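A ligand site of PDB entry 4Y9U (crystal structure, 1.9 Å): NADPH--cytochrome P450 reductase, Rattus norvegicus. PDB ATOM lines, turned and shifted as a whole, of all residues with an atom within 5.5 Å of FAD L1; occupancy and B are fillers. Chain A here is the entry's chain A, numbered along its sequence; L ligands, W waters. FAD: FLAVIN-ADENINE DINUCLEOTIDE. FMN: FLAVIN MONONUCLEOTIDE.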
ATOM      1  N   HIS A 262      22.479   1.892  -5.043  1.00  0.00           N
ATOM      2  CA  HIS A 262      22.989   0.793  -5.810  1.00  0.00           C
ATOM      3  C   HIS A 262      24.354   1.070  -6.355  1.00  0.00           C
ATOM      4  O   HIS A 262      24.677   2.162  -6.606  1.00  0.00           O
ATOM      5  CB  HIS A 262      22.063   0.514  -6.935  1.00  0.00           C
ATOM      6  CG  HIS A 262      20.744  -0.006  -6.500  1.00  0.00           C
ATOM      7  ND1 HIS A 262      19.589   0.705  -6.635  1.00  0.00           N
ATOM      8  CD2 HIS A 262      20.393  -1.175  -5.931  1.00  0.00           C
ATOM      9  CE1 HIS A 262      18.593   0.012  -6.172  1.00  0.00           C
ATOM     10  NE2 HIS A 262      19.050  -1.138  -5.744  1.00  0.00           N
ATOM     11  N   THR A 321      26.282 -13.260 -24.292  1.00  0.00           N
ATOM     12  CA  THR A 321      25.688 -14.332 -23.493  1.00  0.00           C
ATOM     13  C   THR A 321      24.167 -14.405 -23.468  1.00  0.00           C
ATOM     14  O   THR A 321      23.599 -15.459 -23.189  1.00  0.00           O
ATOM     15  CB  THR A 321      26.188 -14.236 -22.056  1.00  0.00           C
ATOM     16  OG1 THR A 321      25.968 -12.902 -21.572  1.00  0.00           O
ATOM     17  CG2 THR A 321      27.685 -14.554 -21.991  1.00  0.00           C
ATOM     18  N   ASN A 322      23.489 -13.292 -23.717  1.00  0.00           N
ATOM     19  CA  ASN A 322      22.031 -13.350 -23.712  1.00  0.00           C
ATOM     20  C   ASN A 322      21.520 -13.845 -25.062  1.00  0.00           C
ATOM     21  O   ASN A 322      22.183 -13.675 -26.083  1.00  0.00           O
ATOM     22  CB  ASN A 322      21.448 -11.988 -23.363  1.00  0.00           C
ATOM     23  CG  ASN A 322      21.631 -11.659 -21.881  1.00  0.00           C
ATOM     24  OD1 ASN A 322      21.403 -12.504 -21.014  1.00  0.00           O
ATOM     25  ND2 ASN A 322      22.046 -10.425 -21.590  1.00  0.00           N
ATOM     26  N   ARG A 367      17.957 -20.806 -23.709  1.00  0.00           N
ATOM     27  CA  ARG A 367      18.982 -19.813 -23.403  1.00  0.00           C
ATOM     28  C   ARG A 367      20.253 -19.987 -24.243  1.00  0.00           C
ATOM     29  O   ARG A 367      21.370 -20.018 -23.722  1.00  0.00           O
ATOM     30  CB  ARG A 367      19.338 -19.886 -21.906  1.00  0.00           C
ATOM     31  CG  ARG A 367      18.185 -19.512 -20.968  1.00  0.00           C
ATOM     32  CD  ARG A 367      17.937 -18.008 -20.954  1.00  0.00           C
ATOM     33  NE  ARG A 367      19.173 -17.269 -20.701  1.00  0.00           N
ATOM     34  CZ  ARG A 367      19.259 -15.944 -20.620  1.00  0.00           C
ATOM     35  NH1 ARG A 367      20.444 -15.382 -20.390  1.00  0.00           N
ATOM     36  NH2 ARG A 367      18.181 -15.177 -20.764  1.00  0.00           N
ATOM     37  N   ARG A 397      25.950  -4.089 -14.383  1.00  0.00           N
ATOM     38  CA  ARG A 397      25.076  -4.849 -13.511  1.00  0.00           C
ATOM     39  C   ARG A 397      24.948  -4.078 -12.193  1.00  0.00           C
ATOM     40  O   ARG A 397      25.936  -3.532 -11.695  1.00  0.00           O
ATOM     41  CB  ARG A 397      25.654  -6.240 -13.239  1.00  0.00           C
ATOM     42  CG  ARG A 397      25.197  -7.346 -14.192  1.00  0.00           C
ATOM     43  CD  ARG A 397      25.670  -7.149 -15.623  1.00  0.00           C
ATOM     44  NE  ARG A 397      25.391  -8.335 -16.448  1.00  0.00           N
ATOM     45  CZ  ARG A 397      25.389  -8.358 -17.780  1.00  0.00           C
ATOM     46  NH1 ARG A 397      25.126  -9.485 -18.428  1.00  0.00           N
ATOM     47  NH2 ARG A 397      25.647  -7.245 -18.474  1.00  0.00           N
ATOM     48  N   TYR A 398      23.739  -4.024 -11.645  1.00  0.00           N
ATOM     49  CA  TYR A 398      23.505  -3.314 -10.393  1.00  0.00           C
ATOM     50  C   TYR A 398      23.430  -4.228  -9.191  1.00  0.00           C
ATOM     51  O   TYR A 398      22.947  -5.367  -9.269  1.00  0.00           O
ATOM     52  CB  TYR A 398      22.216  -2.496 -10.480  1.00  0.00           C
ATOM     53  CG  TYR A 398      22.275  -1.371 -11.474  1.00  0.00           C
ATOM     54  CD1 TYR A 398      22.903  -0.171 -11.157  1.00  0.00           C
ATOM     55  CD2 TYR A 398      21.731  -1.504 -12.749  1.00  0.00           C
ATOM     56  CE1 TYR A 398      23.010   0.859 -12.087  1.00  0.00           C
ATOM     57  CE2 TYR A 398      21.830  -0.492 -13.693  1.00  0.00           C
ATOM     58  CZ  TYR A 398      22.470   0.697 -13.361  1.00  0.00           C
ATOM     59  OH  TYR A 398      22.591   1.709 -14.283  1.00  0.00           O
ATOM     60  N   TYR A 399      23.904  -3.720  -8.053  1.00  0.00           N
ATOM     61  CA  TYR A 399      23.879  -4.474  -6.813  1.00  0.00           C
ATOM     62  C   TYR A 399      23.464  -3.546  -5.691  1.00  0.00           C
ATOM     63  O   TYR A 399      23.729  -2.344  -5.740  1.00  0.00           O
ATOM     64  CB  TYR A 399      25.250  -5.076  -6.541  1.00  0.00           C
ATOM     65  CG  TYR A 399      25.592  -6.122  -7.564  1.00  0.00           C
ATOM     66  CD1 TYR A 399      25.081  -7.413  -7.453  1.00  0.00           C
ATOM     67  CD2 TYR A 399      26.294  -5.789  -8.710  1.00  0.00           C
ATOM     68  CE1 TYR A 399      25.267  -8.357  -8.473  1.00  0.00           C
ATOM     69  CE2 TYR A 399      26.498  -6.721  -9.736  1.00  0.00           C
ATOM     70  CZ  TYR A 399      25.973  -7.996  -9.615  1.00  0.00           C
ATOM     71  OH  TYR A 399      26.129  -8.885 -10.642  1.00  0.00           O
ATOM     72  N   SER A 400      22.770  -4.090  -4.700  1.00  0.00           N
ATOM     73  CA  SER A 400      22.327  -3.265  -3.592  1.00  0.00           C
ATOM     74  C   SER A 400      23.496  -3.134  -2.636  1.00  0.00           C
ATOM     75  O   SER A 400      23.951  -4.124  -2.061  1.00  0.00           O
ATOM     76  CB  SER A 400      21.126  -3.937  -2.913  1.00  0.00           C
ATOM     77  OG  SER A 400      20.053  -4.059  -3.828  1.00  0.00           O
ATOM     78  N   CYS A 415      26.755  -7.940  -1.943  1.00  0.00           N
ATOM     79  CA  CYS A 415      26.310  -9.274  -1.538  1.00  0.00           C
ATOM     80  C   CYS A 415      25.675  -9.858  -2.793  1.00  0.00           C
ATOM     81  O   CYS A 415      24.638  -9.348  -3.264  1.00  0.00           O
ATOM     82  CB  CYS A 415      25.262  -9.192  -0.429  1.00  0.00           C
ATOM     83  SG  CYS A 415      24.500 -10.780  -0.046  1.00  0.00           S
ATOM     84  N   ALA A 416      26.269 -10.912  -3.343  1.00  0.00           N
ATOM     85  CA  ALA A 416      25.733 -11.478  -4.578  1.00  0.00           C
ATOM     86  C   ALA A 416      25.779 -12.997  -4.697  1.00  0.00           C
ATOM     87  O   ALA A 416      26.648 -13.654  -4.136  1.00  0.00           O
ATOM     88  CB  ALA A 416      26.467 -10.868  -5.772  1.00  0.00           C
ATOM     89  N   VAL A 417      24.828 -13.542  -5.439  1.00  0.00           N
ATOM     90  CA  VAL A 417      24.830 -14.974  -5.671  1.00  0.00           C
ATOM     91  C   VAL A 417      25.406 -15.179  -7.069  1.00  0.00           C
ATOM     92  O   VAL A 417      24.976 -14.521  -8.035  1.00  0.00           O
ATOM     93  CB  VAL A 417      23.402 -15.591  -5.570  1.00  0.00           C
ATOM     94  CG1 VAL A 417      22.437 -14.874  -6.508  1.00  0.00           C
ATOM     95  CG2 VAL A 417      23.468 -17.087  -5.875  1.00  0.00           C
ATOM     96  N   VAL A 419      25.890 -16.643 -10.564  1.00  0.00           N
ATOM     97  CA  VAL A 419      24.980 -17.314 -11.485  1.00  0.00           C
ATOM     98  C   VAL A 419      25.709 -18.348 -12.316  1.00  0.00           C
ATOM     99  O   VAL A 419      26.714 -18.055 -12.968  1.00  0.00           O
ATOM    100  CB  VAL A 419      24.304 -16.293 -12.414  1.00  0.00           C
ATOM    101  CG1 VAL A 419      23.320 -17.007 -13.366  1.00  0.00           C
ATOM    102  CG2 VAL A 419      23.562 -15.281 -11.568  1.00  0.00           C
ATOM    103  N   TYR A 421      24.112 -22.069 -14.184  1.00  0.00           N
ATOM    104  CA  TYR A 421      23.012 -23.008 -14.284  1.00  0.00           C
ATOM    105  C   TYR A 421      23.046 -23.846 -15.546  1.00  0.00           C
ATOM    106  O   TYR A 421      23.712 -23.495 -16.523  1.00  0.00           O
ATOM    107  CB  TYR A 421      21.684 -22.241 -14.223  1.00  0.00           C
ATOM    108  CG  TYR A 421      21.502 -21.276 -15.371  1.00  0.00           C
ATOM    109  CD1 TYR A 421      22.092 -20.008 -15.345  1.00  0.00           C
ATOM    110  CD2 TYR A 421      20.794 -21.641 -16.517  1.00  0.00           C
ATOM    111  CE1 TYR A 421      21.983 -19.127 -16.428  1.00  0.00           C
ATOM    112  CE2 TYR A 421      20.661 -20.778 -17.608  1.00  0.00           C
ATOM    113  CZ  TYR A 421      21.261 -19.515 -17.560  1.00  0.00           C
ATOM    114  OH  TYR A 421      21.168 -18.672 -18.644  1.00  0.00           O
ATOM    115  N   GLU A 422      22.308 -24.955 -15.521  1.00  0.00           N
ATOM    116  CA  GLU A 422      22.225 -25.860 -16.651  1.00  0.00           C
ATOM    117  C   GLU A 422      21.130 -25.310 -17.552  1.00  0.00           C
ATOM    118  O   GLU A 422      19.990 -25.128 -17.112  1.00  0.00           O
ATOM    119  CB  GLU A 422      21.821 -27.256 -16.200  1.00  0.00           C
ATOM    120  CG  GLU A 422      22.570 -27.756 -14.993  1.00  0.00           C
ATOM    121  CD  GLU A 422      21.985 -29.046 -14.455  1.00  0.00           C
ATOM    122  OE1 GLU A 422      20.746 -29.111 -14.261  1.00  0.00           O
ATOM    123  OE2 GLU A 422      22.766 -29.998 -14.218  1.00  0.00           O
ATOM    124  N   LYS A 430      27.043 -19.254 -17.582  1.00  0.00           N
ATOM    125  CA  LYS A 430      27.662 -18.539 -16.471  1.00  0.00           C
ATOM    126  C   LYS A 430      27.223 -17.071 -16.508  1.00  0.00           C
ATOM    127  O   LYS A 430      27.128 -16.468 -17.581  1.00  0.00           O
ATOM    128  CB  LYS A 430      29.192 -18.585 -16.578  1.00  0.00           C
ATOM    129  CG  LYS A 430      29.791 -19.976 -16.582  1.00  0.00           C
ATOM    130  CD  LYS A 430      29.769 -20.605 -15.200  1.00  0.00           C
ATOM    131  CE  LYS A 430      30.700 -19.856 -14.246  1.00  0.00           C
ATOM    132  NZ  LYS A 430      32.108 -19.891 -14.723  1.00  0.00           N
ATOM    133  N   GLY A 431      26.945 -16.517 -15.340  1.00  0.00           N
ATOM    134  CA  GLY A 431      26.548 -15.130 -15.257  1.00  0.00           C
ATOM    135  C   GLY A 431      27.773 -14.283 -15.508  1.00  0.00           C
ATOM    136  O   GLY A 431      28.826 -14.510 -14.913  1.00  0.00           O
ATOM    137  N   VAL A 432      27.644 -13.292 -16.375  1.00  0.00           N
ATOM    138  CA  VAL A 432      28.766 -12.438 -16.729  1.00  0.00           C
ATOM    139  C   VAL A 432      29.383 -11.697 -15.543  1.00  0.00           C
ATOM    140  O   VAL A 432      30.530 -11.955 -15.181  1.00  0.00           O
ATOM    141  CB  VAL A 432      28.354 -11.393 -17.796  1.00  0.00           C
ATOM    142  CG1 VAL A 432      29.576 -10.559 -18.207  1.00  0.00           C
ATOM    143  CG2 VAL A 432      27.737 -12.094 -19.005  1.00  0.00           C
ATOM    144  N   ALA A 433      28.630 -10.776 -14.955  1.00  0.00           N
ATOM    145  CA  ALA A 433      29.134  -9.987 -13.842  1.00  0.00           C
ATOM    146  C   ALA A 433      29.532 -10.806 -12.623  1.00  0.00           C
ATOM    147  O   ALA A 433      30.597 -10.577 -12.054  1.00  0.00           O
ATOM    148  CB  ALA A 433      28.125  -8.910 -13.441  1.00  0.00           C
ATOM    149  N   THR A 434      28.684 -11.752 -12.208  1.00  0.00           N
ATOM    150  CA  THR A 434      29.030 -12.536 -11.027  1.00  0.00           C
ATOM    151  C   THR A 434      30.226 -13.469 -11.209  1.00  0.00           C
ATOM    152  O   THR A 434      31.021 -13.639 -10.295  1.00  0.00           O
ATOM    153  CB  THR A 434      27.811 -13.338 -10.489  1.00  0.00           C
ATOM    154  OG1 THR A 434      27.271 -14.169 -11.518  1.00  0.00           O
ATOM    155  CG2 THR A 434      26.729 -12.379  -9.990  1.00  0.00           C
ATOM    156  N   SER A 435      30.381 -14.060 -12.402  1.00  0.00           N
ATOM    157  CA  SER A 435      31.532 -14.937 -12.625  1.00  0.00           C
ATOM    158  C   SER A 435      32.816 -14.097 -12.577  1.00  0.00           C
ATOM    159  O   SER A 435      33.845 -14.529 -12.040  1.00  0.00           O
ATOM    160  CB  SER A 435      31.460 -15.630 -13.994  1.00  0.00           C
ATOM    161  OG  SER A 435      30.387 -16.559 -14.035  1.00  0.00           O
ATOM    162  N   ARG A 457      24.447   4.640  -8.156  1.00  0.00           N
ATOM    163  CA  ARG A 457      23.195   5.189  -8.631  1.00  0.00           C
ATOM    164  C   ARG A 457      22.341   5.436  -7.405  1.00  0.00           C
ATOM    165  O   ARG A 457      22.043   4.515  -6.651  1.00  0.00           O
ATOM    166  CB  ARG A 457      22.470   4.235  -9.572  1.00  0.00           C
ATOM    167  CG  ARG A 457      21.206   4.848 -10.182  1.00  0.00           C
ATOM    168  CD  ARG A 457      20.520   3.873 -11.118  1.00  0.00           C
ATOM    169  NE  ARG A 457      20.117   2.664 -10.416  1.00  0.00           N
ATOM    170  CZ  ARG A 457      19.617   1.578 -11.006  1.00  0.00           C
ATOM    171  NH1 ARG A 457      19.455   1.555 -12.327  1.00  0.00           N
ATOM    172  NH2 ARG A 457      19.293   0.514 -10.283  1.00  0.00           N
ATOM    173  N   THR A 478      19.609 -13.150  -1.021  1.00  0.00           N
ATOM    174  CA  THR A 478      20.402 -11.955  -1.307  1.00  0.00           C
ATOM    175  C   THR A 478      19.614 -10.674  -1.043  1.00  0.00           C
ATOM    176  O   THR A 478      20.141  -9.573  -1.155  1.00  0.00           O
ATOM    177  CB  THR A 478      20.915 -11.932  -2.773  1.00  0.00           C
ATOM    178  OG1 THR A 478      19.825 -12.161  -3.679  1.00  0.00           O
ATOM    179  CG2 THR A 478      21.987 -12.989  -2.970  1.00  0.00           C
ATOM    180  N   ALA A 481      20.989  -7.929   1.432  1.00  0.00           N
ATOM    181  CA  ALA A 481      21.982  -6.927   1.033  1.00  0.00           C
ATOM    182  C   ALA A 481      21.909  -5.503   1.602  1.00  0.00           C
ATOM    183  O   ALA A 481      22.779  -5.093   2.370  1.00  0.00           O
ATOM    184  CB  ALA A 481      22.046  -6.873  -0.502  1.00  0.00           C
ATOM    185  N   ASP A 618      13.023  -2.953  -3.169  1.00  0.00           N
ATOM    186  CA  ASP A 618      14.295  -3.054  -3.864  1.00  0.00           C
ATOM    187  C   ASP A 618      14.294  -4.517  -4.282  1.00  0.00           C
ATOM    188  O   ASP A 618      14.933  -5.359  -3.662  1.00  0.00           O
ATOM    189  CB  ASP A 618      15.474  -2.761  -2.942  1.00  0.00           C
ATOM    190  CG  ASP A 618      16.815  -2.898  -3.647  1.00  0.00           C
ATOM    191  OD1 ASP A 618      16.846  -2.886  -4.899  1.00  0.00           O
ATOM    192  OD2 ASP A 618      17.849  -3.020  -2.958  1.00  0.00           O
ATOM    193  N   VAL A 619      13.515  -4.801  -5.317  1.00  0.00           N
ATOM    194  CA  VAL A 619      13.401  -6.159  -5.805  1.00  0.00           C
ATOM    195  C   VAL A 619      13.833  -6.256  -7.260  1.00  0.00           C
ATOM    196  O   VAL A 619      13.784  -5.272  -8.005  1.00  0.00           O
ATOM    197  CB  VAL A 619      11.959  -6.685  -5.667  1.00  0.00           C
ATOM    198  CG1 VAL A 619      11.615  -6.841  -4.198  1.00  0.00           C
ATOM    199  CG2 VAL A 619      10.964  -5.720  -6.337  1.00  0.00           C
ATOM    200  N   TRP A 620      14.283  -7.441  -7.656  1.00  0.00           N
ATOM    201  CA  TRP A 620      14.730  -7.683  -9.011  1.00  0.00           C
ATOM    202  C   TRP A 620      14.419  -9.136  -9.341  1.00  0.00           C
ATOM    203  O   TRP A 620      14.046  -9.925  -8.468  1.00  0.00           O
ATOM    204  CB  TRP A 620      16.244  -7.409  -9.127  1.00  0.00           C
ATOM    205  CG  TRP A 620      17.083  -8.250  -8.205  1.00  0.00           C
ATOM    206  CD1 TRP A 620      17.604  -9.493  -8.463  1.00  0.00           C
ATOM    207  CD2 TRP A 620      17.478  -7.917  -6.860  1.00  0.00           C
ATOM    208  NE1 TRP A 620      18.291  -9.955  -7.356  1.00  0.00           N
ATOM    209  CE2 TRP A 620      18.229  -9.017  -6.369  1.00  0.00           C
ATOM    210  CE3 TRP A 620      17.276  -6.807  -6.031  1.00  0.00           C
ATOM    211  CZ2 TRP A 620      18.777  -9.024  -5.074  1.00  0.00           C
ATOM    212  CZ3 TRP A 620      17.819  -6.819  -4.748  1.00  0.00           C
ATOM    213  CH2 TRP A 620      18.558  -7.928  -4.280  1.00  0.00           C
ATOM    214  N   SER A 621      14.559  -9.506 -10.606  1.00  0.00           N
ATOM    215  CA  SER A 621      14.275 -10.875 -10.990  1.00  0.00           C
ATOM    216  C   SER A 621      15.392 -11.457 -11.845  1.00  0.00           C
ATOM    217  O   SER A 621      15.100 -11.907 -12.969  1.00  0.00           O
ATOM    218  CB  SER A 621      12.939 -10.946 -11.739  1.00  0.00           C
ATOM    219  OG  SER A 621      12.961 -10.126 -12.887  1.00  0.00           O
ATOM    220  OXT SER A 621      16.544 -11.444 -11.367  1.00  0.00           O
HETATM  221  PA  FAD L   1      23.798 -12.478 -16.437  1.00  0.00           P
HETATM  222  O1A FAD L   1      24.873 -12.924 -17.351  1.00  0.00           O
HETATM  223  O2A FAD L   1      23.312 -11.084 -16.522  1.00  0.00           O
HETATM  224  O5B FAD L   1      22.548 -13.479 -16.605  1.00  0.00           O
HETATM  225  C5B FAD L   1      21.320 -13.227 -15.909  1.00  0.00           C
HETATM  226  C4B FAD L   1      20.213 -14.027 -16.584  1.00  0.00           C
HETATM  227  O4B FAD L   1      20.481 -15.431 -16.514  1.00  0.00           O
HETATM  228  C3B FAD L   1      18.895 -13.928 -15.834  1.00  0.00           C
HETATM  229  O3B FAD L   1      18.286 -12.665 -16.141  1.00  0.00           O
HETATM  230  C2B FAD L   1      18.153 -15.025 -16.561  1.00  0.00           C
HETATM  231  O2B FAD L   1      17.726 -14.547 -17.841  1.00  0.00           O
HETATM  232  C1B FAD L   1      19.224 -16.098 -16.743  1.00  0.00           C
HETATM  233  N9A FAD L   1      19.122 -17.155 -15.730  1.00  0.00           N
HETATM  234  C8A FAD L   1      19.613 -17.096 -14.333  1.00  0.00           C
HETATM  235  N7A FAD L   1      19.257 -18.459 -13.869  1.00  0.00           N
HETATM  236  C5A FAD L   1      18.677 -19.116 -14.863  1.00  0.00           C
HETATM  237  C6A FAD L   1      18.209 -20.365 -14.889  1.00  0.00           C
HETATM  238  N6A FAD L   1      18.403 -21.081 -13.786  1.00  0.00           N
HETATM  239  N1A FAD L   1      17.541 -20.866 -15.936  1.00  0.00           N
HETATM  240  C2A FAD L   1      17.319 -20.043 -17.049  1.00  0.00           C
HETATM  241  N3A FAD L   1      17.799 -18.730 -16.980  1.00  0.00           N
HETATM  242  C4A FAD L   1      18.467 -18.306 -15.904  1.00  0.00           C
HETATM  243  N1  FAD L   1      21.953  -9.443  -7.458  1.00  0.00           N
HETATM  244  C2  FAD L   1      22.622  -9.859  -6.303  1.00  0.00           C
HETATM  245  O2  FAD L   1      23.088 -11.001  -6.248  1.00  0.00           O
HETATM  246  N3  FAD L   1      22.696  -9.008  -5.197  1.00  0.00           N
HETATM  247  C4  FAD L   1      22.110  -7.742  -5.242  1.00  0.00           C
HETATM  248  O4  FAD L   1      22.275  -6.966  -4.301  1.00  0.00           O
HETATM  249  C4X FAD L   1      21.432  -7.340  -6.387  1.00  0.00           C
HETATM  250  N5  FAD L   1      20.750  -6.175  -6.388  1.00  0.00           N
HETATM  251  C5X FAD L   1      20.108  -5.783  -7.496  1.00  0.00           C
HETATM  252  C6  FAD L   1      19.479  -4.543  -7.518  1.00  0.00           C
HETATM  253  C7  FAD L   1      18.872  -4.091  -8.684  1.00  0.00           C
HETATM  254  C7M FAD L   1      18.352  -2.798  -8.730  1.00  0.00           C
HETATM  255  C8  FAD L   1      18.877  -4.892  -9.823  1.00  0.00           C
HETATM  256  C8M FAD L   1      18.286  -4.441 -10.996  1.00  0.00           C
HETATM  257  C9  FAD L   1      19.503  -6.125  -9.793  1.00  0.00           C
HETATM  258  C9A FAD L   1      20.143  -6.566  -8.640  1.00  0.00           C
HETATM  259  N10 FAD L   1      20.809  -7.730  -8.632  1.00  0.00           N
HETATM  260  C10 FAD L   1      21.345  -8.177  -7.484  1.00  0.00           C
HETATM  261  C1' FAD L   1      20.890  -8.590  -9.843  1.00  0.00           C
HETATM  262  C2' FAD L   1      22.174  -8.270 -10.615  1.00  0.00           C
HETATM  263  O2' FAD L   1      22.089  -6.950 -11.149  1.00  0.00           O
HETATM  264  C3' FAD L   1      22.405  -9.252 -11.767  1.00  0.00           C
HETATM  265  O3' FAD L   1      21.237  -9.345 -12.590  1.00  0.00           O
HETATM  266  C4' FAD L   1      22.778 -10.641 -11.246  1.00  0.00           C
HETATM  267  O4' FAD L   1      23.901 -10.550 -10.368  1.00  0.00           O
HETATM  268  C5' FAD L   1      23.139 -11.551 -12.431  1.00  0.00           C
HETATM  269  O5' FAD L   1      24.111 -10.899 -13.250  1.00  0.00           O
HETATM  270  P   FAD L   1      25.180 -11.738 -14.122  1.00  0.00           P
HETATM  271  O1P FAD L   1      26.045 -12.511 -13.198  1.00  0.00           O
HETATM  272  O2P FAD L   1      25.819 -10.797 -15.067  1.00  0.00           O
HETATM  273  O3P FAD L   1      24.245 -12.776 -14.921  1.00  0.00           O
HETATM  274  N1  FMN L   2       8.144  -2.567 -15.319  1.00  0.00           N
HETATM  275  C2  FMN L   2       6.946  -1.987 -15.090  1.00  0.00           C
HETATM  276  O2  FMN L   2       6.013  -2.110 -15.881  1.00  0.00           O
HETATM  277  N3  FMN L   2       6.834  -1.239 -13.929  1.00  0.00           N
HETATM  278  C4  FMN L   2       7.822  -1.020 -12.952  1.00  0.00           C
HETATM  279  O4  FMN L   2       7.480  -0.331 -12.006  1.00  0.00           O
HETATM  280  C4A FMN L   2       9.076  -1.645 -13.174  1.00  0.00           C
HETATM  281  N5  FMN L   2      10.087  -1.463 -12.210  1.00  0.00           N
HETATM  282  C5A FMN L   2      11.286  -2.106 -12.507  1.00  0.00           C
HETATM  283  C6  FMN L   2      12.331  -1.953 -11.532  1.00  0.00           C
HETATM  284  C7  FMN L   2      13.604  -2.566 -11.701  1.00  0.00           C
HETATM  285  C7M FMN L   2      14.615  -2.307 -10.568  1.00  0.00           C
HETATM  286  C8  FMN L   2      13.890  -3.405 -12.911  1.00  0.00           C
HETATM  287  C8M FMN L   2      15.083  -4.049 -13.196  1.00  0.00           C
HETATM  288  C9  FMN L   2      12.892  -3.561 -13.866  1.00  0.00           C
HETATM  289  C9A FMN L   2      11.567  -2.932 -13.703  1.00  0.00           C
HETATM  290  N10 FMN L   2      10.460  -3.064 -14.664  1.00  0.00           N
HETATM  291  C10 FMN L   2       9.161  -2.403 -14.393  1.00  0.00           C
HETATM  292  C1' FMN L   2      10.607  -3.843 -15.897  1.00  0.00           C
HETATM  293  C2' FMN L   2      11.159  -3.012 -17.098  1.00  0.00           C
HETATM  294  O2' FMN L   2      10.233  -1.890 -17.364  1.00  0.00           O
HETATM  295  C3' FMN L   2      11.286  -3.889 -18.333  1.00  0.00           C
HETATM  296  O3' FMN L   2      12.212  -4.954 -18.006  1.00  0.00           O
HETATM  297  C4' FMN L   2      11.827  -3.012 -19.538  1.00  0.00           C
HETATM  298  O4' FMN L   2      11.846  -3.997 -20.611  1.00  0.00           O
HETATM  299  C5' FMN L   2      13.272  -2.544 -19.363  1.00  0.00           C
HETATM  300  O5' FMN L   2      13.755  -1.711 -20.507  1.00  0.00           O
HETATM  301  P   FMN L   2      15.198  -1.079 -20.688  1.00  0.00           P
HETATM  302  O1P FMN L   2      16.224  -2.136 -20.888  1.00  0.00           O
HETATM  303  O2P FMN L   2      15.340  -0.091 -19.485  1.00  0.00           O
HETATM  304  O3P FMN L   2      15.010  -0.309 -22.081  1.00  0.00           O
HETATM  305  O   HOH W   1      24.890 -15.633 -18.881  1.00  0.00           O
HETATM  306  O   HOH W   2      17.907 -14.784 -12.353  1.00  0.00           O
HETATM  307  O   HOH W   3      20.616 -18.462 -11.319  1.00  0.00           O
HETATM  308  O   HOH W   4      22.367 -16.217 -18.454  1.00  0.00           O
HETATM  309  O   HOH W   5      21.608  -5.460 -13.216  1.00  0.00           O
HETATM  310  O   HOH W   6      22.050  -9.202 -15.223  1.00  0.00           O
HETATM  311  O   HOH W   7      19.054 -11.048 -18.855  1.00  0.00           O
HETATM  312  O   HOH W   8      21.794  -9.953 -18.670  1.00  0.00           O
HETATM  313  O   HOH W   9      24.775  -6.370  -3.139  1.00  0.00           O
HETATM  314  O   HOH W  10      23.194 -12.353  -8.553  1.00  0.00           O
HETATM  315  O   HOH W  11      19.888 -12.019  -6.664  1.00  0.00           O
HETATM  316  O   HOH W  12      24.007 -12.705 -19.932  1.00  0.00           O
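The guanidinium group (NH2) of Arg 367 is in hydrogen-bond range of an oxygen (O2B) of FAD L1 (3.0 Å).
The side-chain hydroxyl (OG1) of Thr 434 is in hydrogen-bond range of an oxygen (O1P) of FAD L1 (2.7 Å).
The side-chain hydroxyl of Ser 400 sits at hydrogen-bond distance from a nitrogen (N5) of FAD L1 (3.4 Å).
O4 of FAD L1 lies within hydrogen-bond range of N of Ser 400 (2.9 Å).
The guanidinium group (NE) of Arg 397 is in salt-bridge range of an oxygen (O2P) of FAD L1 (2.9 Å).
O of Cys 415 lies within hydrogen-bond range of N3 of FAD L1, at 2.8 Å.
The backbone NH (N) of Thr 434 lies within hydrogen-bond range of an oxygen (O1P) of FAD L1, at 2.9 Å.
The backbone NH (N) of Ala 433 is in hydrogen-bond range of an oxygen (O2P) of FAD L1, 2.8 Å away.
N of Val 432 sits at hydrogen-bond distance from O1A of FAD L1.
An oxygen (O2) of FAD L1 is in hydrogen-bond range of the backbone NH (N) of Val 417 (3.2 Å).
The backbone carbonyl oxygen of Tyr 398 sits at hydrogen-bond distance from an oxygen (O2') of FAD L1 (2.6 Å).
OH of Tyr 399 sits at hydrogen-bond distance from O4' of FAD L1, 2.8 Å away.
N of Tyr 398 lies within hydrogen-bond range of O2' of FAD L1, at 3.4 Å.
The side-chain hydroxyl (OH) of Tyr 421 lies within hydrogen-bond range of the guanidinium group (NE) of Arg 367, 3.2 Å away.
OG of Ser 435 sits at hydrogen-bond distance from O of Gly 431, at 2.7 Å.
The backbone carbonyl oxygen (O) of Val 419 is in hydrogen-bond range of the backbone NH (N) of Gly 431.
NE2 of His 262 is in hydrogen-bond range of OD1 of Asp 618, at 2.9 Å.
The side-chain carboxylate of Asp 618 lies within hydrogen-bond range of the side-chain hydroxyl of Ser 400 (2.6 Å).
The backbone NH (N) of Val 419 is in hydrogen-bond range of the side-chain hydroxyl (OG1) of Thr 434 (3.0 Å).
The backbone carbonyl oxygen (O) of His 262 sits at hydrogen-bond distance from the backbone NH (N) of Arg 457 (2.9 Å).
The guanidinium group (NH1) of Arg 367 sits at hydrogen-bond distance from the side-chain amide oxygen (OD1) of Asn 322, at 3.1 Å.
Merely in contact with FAD L1: His 262, Ala 416, Val 419, Tyr 421, Gly 431, Arg 457, Thr 478, Ala 481 and Trp 620.
The nearest printed residue that does not touch FAD L1 is Asp 618 (4.1 Å).
Water W5 bridges O2' of FAD L1 (2.6 Å) and N of Tyr 398 (3.0 Å).
Water W10 bridges an oxygen (O4') of FAD L1 (2.7 Å) and the backbone carbonyl oxygen of Val 417 (2.9 Å).
Water W12 lies within hydrogen-bond range of OG1 of Thr 321 (2.6 Å), O1A of FAD L1 (2.7 Å) and OD1 of Asn 322 (2.8 Å).
Water W4 lies within hydrogen-bond range of OH of Tyr 421 (2.7 Å), O4B of FAD L1 (2.8 Å) and NH1 of Arg 367 (2.9 Å).
Water W8 lies within hydrogen-bond range of O2A of FAD L1 (2.9 Å), ND2 of Asn 322 (3.0 Å) and NH1 of Arg 397 (3.4 Å).
Water W1 bridges the backbone carbonyl oxygen of Lys 430 and an oxygen (O1A) of FAD L1.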
